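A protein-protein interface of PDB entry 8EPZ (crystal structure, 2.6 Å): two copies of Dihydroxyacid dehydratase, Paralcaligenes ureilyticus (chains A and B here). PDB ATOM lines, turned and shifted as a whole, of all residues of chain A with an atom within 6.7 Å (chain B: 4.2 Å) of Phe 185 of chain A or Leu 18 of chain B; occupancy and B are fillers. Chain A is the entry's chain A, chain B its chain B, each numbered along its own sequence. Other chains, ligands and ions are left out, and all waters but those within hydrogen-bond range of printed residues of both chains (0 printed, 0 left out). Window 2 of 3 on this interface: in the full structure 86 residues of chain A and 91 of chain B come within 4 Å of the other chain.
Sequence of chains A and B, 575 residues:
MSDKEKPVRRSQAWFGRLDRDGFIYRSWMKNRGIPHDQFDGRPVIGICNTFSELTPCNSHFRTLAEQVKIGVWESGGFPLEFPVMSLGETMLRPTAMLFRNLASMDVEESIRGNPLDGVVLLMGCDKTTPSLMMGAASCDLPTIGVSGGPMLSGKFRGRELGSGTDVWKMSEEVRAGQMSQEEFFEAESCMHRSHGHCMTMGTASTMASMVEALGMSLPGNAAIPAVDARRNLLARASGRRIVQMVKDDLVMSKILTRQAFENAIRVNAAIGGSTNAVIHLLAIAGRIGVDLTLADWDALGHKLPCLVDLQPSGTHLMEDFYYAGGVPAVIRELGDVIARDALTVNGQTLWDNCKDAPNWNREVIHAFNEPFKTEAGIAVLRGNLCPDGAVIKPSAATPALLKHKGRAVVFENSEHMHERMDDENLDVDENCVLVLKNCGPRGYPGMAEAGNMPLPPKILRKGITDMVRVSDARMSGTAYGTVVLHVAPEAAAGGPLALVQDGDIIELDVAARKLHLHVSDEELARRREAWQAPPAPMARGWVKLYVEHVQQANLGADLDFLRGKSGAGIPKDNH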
ATOM      1  N   MET A 170      24.770  -3.377  16.598  1.00  0.00           N
ATOM      2  CA  MET A 170      23.722  -2.382  16.822  1.00  0.00           C
ATOM      3  C   MET A 170      22.344  -3.029  16.878  1.00  0.00           C
ATOM      4  O   MET A 170      21.486  -2.595  17.655  1.00  0.00           O
ATOM      5  CB  MET A 170      23.756  -1.303  15.737  1.00  0.00           C
ATOM      6  CG  MET A 170      24.970  -0.383  15.799  1.00  0.00           C
ATOM      7  SD  MET A 170      24.931   0.923  14.554  1.00  0.00           S
ATOM      8  CE  MET A 170      23.847   0.201  13.324  1.00  0.00           C
ATOM      9  N   SER A 180      18.019   3.092  19.864  1.00  0.00           N
ATOM     10  CA  SER A 180      16.774   3.463  19.211  1.00  0.00           C
ATOM     11  C   SER A 180      16.528   2.562  18.009  1.00  0.00           C
ATOM     12  O   SER A 180      17.461   2.121  17.331  1.00  0.00           O
ATOM     13  CB  SER A 180      16.819   4.921  18.755  1.00  0.00           C
ATOM     14  OG  SER A 180      17.380   5.747  19.758  1.00  0.00           O
ATOM     15  N   GLN A 181      15.251   2.273  17.756  1.00  0.00           N
ATOM     16  CA  GLN A 181      14.897   1.566  16.534  1.00  0.00           C
ATOM     17  C   GLN A 181      15.171   2.397  15.286  1.00  0.00           C
ATOM     18  O   GLN A 181      15.155   1.846  14.183  1.00  0.00           O
ATOM     19  CB  GLN A 181      13.425   1.153  16.575  1.00  0.00           C
ATOM     20  N   GLU A 182      15.429   3.696  15.436  1.00  0.00           N
ATOM     21  CA  GLU A 182      15.705   4.596  14.323  1.00  0.00           C
ATOM     22  C   GLU A 182      17.186   4.920  14.170  1.00  0.00           C
ATOM     23  O   GLU A 182      17.675   5.007  13.037  1.00  0.00           O
ATOM     24  CB  GLU A 182      14.910   5.895  14.484  1.00  0.00           C
ATOM     25  CG  GLU A 182      14.959   6.808  13.270  1.00  0.00           C
ATOM     26  CD  GLU A 182      14.151   6.274  12.099  1.00  0.00           C
ATOM     27  OE1 GLU A 182      13.402   5.291  12.284  1.00  0.00           O
ATOM     28  OE2 GLU A 182      14.264   6.842  10.993  1.00  0.00           O
ATOM     29  N   GLU A 183      17.904   5.108  15.287  1.00  0.00           N
ATOM     30  CA  GLU A 183      19.355   5.279  15.231  1.00  0.00           C
ATOM     31  C   GLU A 183      20.002   4.157  14.427  1.00  0.00           C
ATOM     32  O   GLU A 183      21.016   4.362  13.746  1.00  0.00           O
ATOM     33  CB  GLU A 183      19.923   5.323  16.652  1.00  0.00           C
ATOM     34  CG  GLU A 183      21.408   5.653  16.748  1.00  0.00           C
ATOM     35  CD  GLU A 183      21.933   5.589  18.171  1.00  0.00           C
ATOM     36  OE1 GLU A 183      23.039   5.041  18.373  1.00  0.00           O
ATOM     37  OE2 GLU A 183      21.238   6.077  19.087  1.00  0.00           O
ATOM     38  N   PHE A 184      19.406   2.965  14.490  1.00  0.00           N
ATOM     39  CA  PHE A 184      19.814   1.854  13.639  1.00  0.00           C
ATOM     40  C   PHE A 184      19.697   2.216  12.161  1.00  0.00           C
ATOM     41  O   PHE A 184      20.645   2.037  11.388  1.00  0.00           O
ATOM     42  CB  PHE A 184      18.957   0.634  13.982  1.00  0.00           C
ATOM     43  CG  PHE A 184      19.223  -0.565  13.129  1.00  0.00           C
ATOM     44  CD1 PHE A 184      20.459  -1.183  13.137  1.00  0.00           C
ATOM     45  CD2 PHE A 184      18.212  -1.103  12.349  1.00  0.00           C
ATOM     46  CE1 PHE A 184      20.694  -2.298  12.362  1.00  0.00           C
ATOM     47  CE2 PHE A 184      18.440  -2.217  11.573  1.00  0.00           C
ATOM     48  CZ  PHE A 184      19.682  -2.820  11.585  1.00  0.00           C
ATOM     49  N   PHE A 185      18.541   2.746  11.750  1.00  0.00           N
ATOM     50  CA  PHE A 185      18.290   3.017  10.337  1.00  0.00           C
ATOM     51  C   PHE A 185      18.862   4.343   9.855  1.00  0.00           C
ATOM     52  O   PHE A 185      18.866   4.584   8.642  1.00  0.00           O
ATOM     53  CB  PHE A 185      16.789   2.993  10.044  1.00  0.00           C
ATOM     54  CG  PHE A 185      16.159   1.650  10.241  1.00  0.00           C
ATOM     55  CD1 PHE A 185      16.478   0.592   9.408  1.00  0.00           C
ATOM     56  CD2 PHE A 185      15.243   1.450  11.254  1.00  0.00           C
ATOM     57  CE1 PHE A 185      15.897  -0.645   9.592  1.00  0.00           C
ATOM     58  CE2 PHE A 185      14.661   0.218  11.444  1.00  0.00           C
ATOM     59  CZ  PHE A 185      14.988  -0.831  10.612  1.00  0.00           C
ATOM     60  N   GLU A 186      19.321   5.212  10.755  1.00  0.00           N
ATOM     61  CA  GLU A 186      19.959   6.448  10.310  1.00  0.00           C
ATOM     62  C   GLU A 186      21.418   6.225   9.946  1.00  0.00           C
ATOM     63  O   GLU A 186      21.938   6.885   9.038  1.00  0.00           O
ATOM     64  CB  GLU A 186      19.828   7.525  11.383  1.00  0.00           C
ATOM     65  CG  GLU A 186      18.387   7.780  11.787  1.00  0.00           C
ATOM     66  CD  GLU A 186      18.154   9.180  12.314  1.00  0.00           C
ATOM     67  OE1 GLU A 186      17.081   9.409  12.908  1.00  0.00           O
ATOM     68  OE2 GLU A 186      19.034  10.052  12.131  1.00  0.00           O
ATOM     69  N   ALA A 187      22.084   5.290  10.624  1.00  0.00           N
ATOM     70  CA  ALA A 187      23.421   4.857  10.243  1.00  0.00           C
ATOM     71  C   ALA A 187      23.430   4.087   8.930  1.00  0.00           C
ATOM     72  O   ALA A 187      24.508   3.701   8.465  1.00  0.00           O
ATOM     73  CB  ALA A 187      24.018   3.991  11.353  1.00  0.00           C
ATOM     74  N   GLU A 188      22.258   3.867   8.333  1.00  0.00           N
ATOM     75  CA  GLU A 188      22.146   3.072   7.114  1.00  0.00           C
ATOM     76  C   GLU A 188      22.962   3.680   5.979  1.00  0.00           C
ATOM     77  O   GLU A 188      23.846   3.029   5.408  1.00  0.00           O
ATOM     78  CB  GLU A 188      20.671   2.952   6.728  1.00  0.00           C
ATOM     79  CG  GLU A 188      20.322   1.775   5.845  1.00  0.00           C
ATOM     80  CD  GLU A 188      18.837   1.706   5.546  1.00  0.00           C
ATOM     81  OE1 GLU A 188      18.094   1.079   6.333  1.00  0.00           O
ATOM     82  OE2 GLU A 188      18.409   2.294   4.529  1.00  0.00           O
ATOM     83  N   SER A 189      22.676   4.938   5.644  1.00  0.00           N
ATOM     84  CA  SER A 189      23.391   5.634   4.584  1.00  0.00           C
ATOM     85  C   SER A 189      24.766   6.130   5.010  1.00  0.00           C
ATOM     86  O   SER A 189      25.576   6.475   4.143  1.00  0.00           O
ATOM     87  CB  SER A 189      22.555   6.811   4.083  1.00  0.00           C
ATOM     88  OG  SER A 189      22.139   7.633   5.161  1.00  0.00           O
ATOM     89  N   GLY B  16      11.845  -2.930   1.847  1.00  0.00           N
ATOM     90  CA  GLY B  16      10.817  -2.338   2.680  1.00  0.00           C
ATOM     91  C   GLY B  16      10.871  -2.800   4.121  1.00  0.00           C
ATOM     92  O   GLY B  16      10.097  -2.336   4.964  1.00  0.00           O
ATOM     93  N   ARG B  17      11.793  -3.715   4.413  1.00  0.00           N
ATOM     94  CA  ARG B  17      11.864  -4.323   5.734  1.00  0.00           C
ATOM     95  C   ARG B  17      12.398  -3.327   6.755  1.00  0.00           C
ATOM     96  O   ARG B  17      13.467  -2.739   6.565  1.00  0.00           O
ATOM     97  CB  ARG B  17      12.750  -5.566   5.689  1.00  0.00           C
ATOM     98  CG  ARG B  17      12.252  -6.642   4.742  1.00  0.00           C
ATOM     99  CD  ARG B  17      11.334  -7.625   5.447  1.00  0.00           C
ATOM    100  NE  ARG B  17      12.014  -8.301   6.549  1.00  0.00           N
ATOM    101  CZ  ARG B  17      12.822  -9.345   6.398  1.00  0.00           C
ATOM    102  NH1 ARG B  17      13.059  -9.835   5.188  1.00  0.00           N
ATOM    103  NH2 ARG B  17      13.399  -9.898   7.458  1.00  0.00           N
ATOM    104  N   LEU B  18      11.654  -3.142   7.838  1.00  0.00           N
ATOM    105  CA  LEU B  18      12.090  -2.288   8.944  1.00  0.00           C
ATOM    106  C   LEU B  18      12.649  -3.120  10.090  1.00  0.00           C
ATOM    107  O   LEU B  18      12.283  -2.951  11.253  1.00  0.00           O
ATOM    108  CB  LEU B  18      10.939  -1.407   9.417  1.00  0.00           C
ATOM    109  CG  LEU B  18      10.306  -0.509   8.354  1.00  0.00           C
ATOM    110  CD1 LEU B  18       8.834  -0.849   8.196  1.00  0.00           C
ATOM    111  CD2 LEU B  18      10.485   0.962   8.699  1.00  0.00           C
ATOM    112  N   ASP B  19      13.550  -4.045   9.760  1.00  0.00           N
ATOM    113  CA  ASP B  19      14.196  -4.882  10.762  1.00  0.00           C
ATOM    114  C   ASP B  19      15.706  -4.889  10.555  1.00  0.00           C
ATOM    115  O   ASP B  19      16.237  -4.072   9.796  1.00  0.00           O
ATOM    116  CB  ASP B  19      13.637  -6.307  10.717  1.00  0.00           C
ATOM    117  CG  ASP B  19      13.447  -6.822   9.299  1.00  0.00           C
ATOM    118  OD1 ASP B  19      14.407  -6.759   8.503  1.00  0.00           O
ATOM    119  OD2 ASP B  19      12.339  -7.303   8.979  1.00  0.00           O
ATOM    120  N   ARG B  26      19.511  -2.493   2.249  1.00  0.00           N
ATOM    121  CA  ARG B  26      19.501  -1.089   1.858  1.00  0.00           C
ATOM    122  C   ARG B  26      20.843  -0.396   2.025  1.00  0.00           C
ATOM    123  O   ARG B  26      21.216   0.419   1.179  1.00  0.00           O
ATOM    124  CB  ARG B  26      18.438  -0.325   2.661  1.00  0.00           C
ATOM    125  CG  ARG B  26      17.236   0.120   1.836  1.00  0.00           C
ATOM    126  CD  ARG B  26      16.169   0.810   2.685  1.00  0.00           C
ATOM    127  NE  ARG B  26      15.226  -0.127   3.293  1.00  0.00           N
ATOM    128  CZ  ARG B  26      15.205  -0.438   4.584  1.00  0.00           C
ATOM    129  NH1 ARG B  26      16.076   0.114   5.417  1.00  0.00           N
ATOM    130  NH2 ARG B  26      14.310  -1.300   5.047  1.00  0.00           N
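The side-chain carboxylate (OE1) of Glu 188 of chain A lies within salt-bridge range of the guanidinium group (NH1) of Arg 26 of chain B (2.4 Å).
Among the printed residues, pairs that only touch across the chains: Phe 185 of chain A with Leu 18 of chain B (3.3 Å), Phe 184 of chain A with Asp 19 of chain B (3.4 Å) and Phe 185 of chain A with Asp 19 of chain B (3.4 Å).
Of chain B, only Leu 18 and Asp 19 come within 4 Å of Phe 185 of chain A.
Leu 18 of chain B touches just one residue of chain A: Phe 185 (3.3 Å).
Printed residues of chain A within 4 Å of Asp 19 of chain B: Phe 184 (3.4 Å) and Phe 185 (3.4 Å).
Of the printed residues of chain B, Phe 184 of chain A touches Asp 19.
Of the printed residues of chain B, Glu 188 of chain A touches Arg 26 (2.4 Å).
Of the printed residues of chain A, Arg 26 of chain B touches Glu 188.
Glu 183 of chain A touches none of the printed residues of chain B.
Arg 17 of chain B touches none of the printed residues of chain A.
The nearest residue of chain B that does not touch Phe 185 of chain A is Arg 26 of chain B (4.04 Å).
The nearest residue of chain A that does not touch Leu 18 of chain B is Phe 184 of chain A (6.0 Å).
The nearest printed residue of chain B that does not touch Phe 184 of chain A is Leu 18 of chain B (6.0 Å).
The side-chain carboxylate (OD2) of Asp 19 of chain B is in salt-bridge range of the guanidinium group (NE) of Arg 17 of chain B (2.6 Å).
No position is printed for both chains.
Of the 4 pairs that touch across the chains among the printed residues, none has its exchanged pair printed and touching as well.
Along chain A the printed residues that touch a printed residue of chain B span positions 184 to 188.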
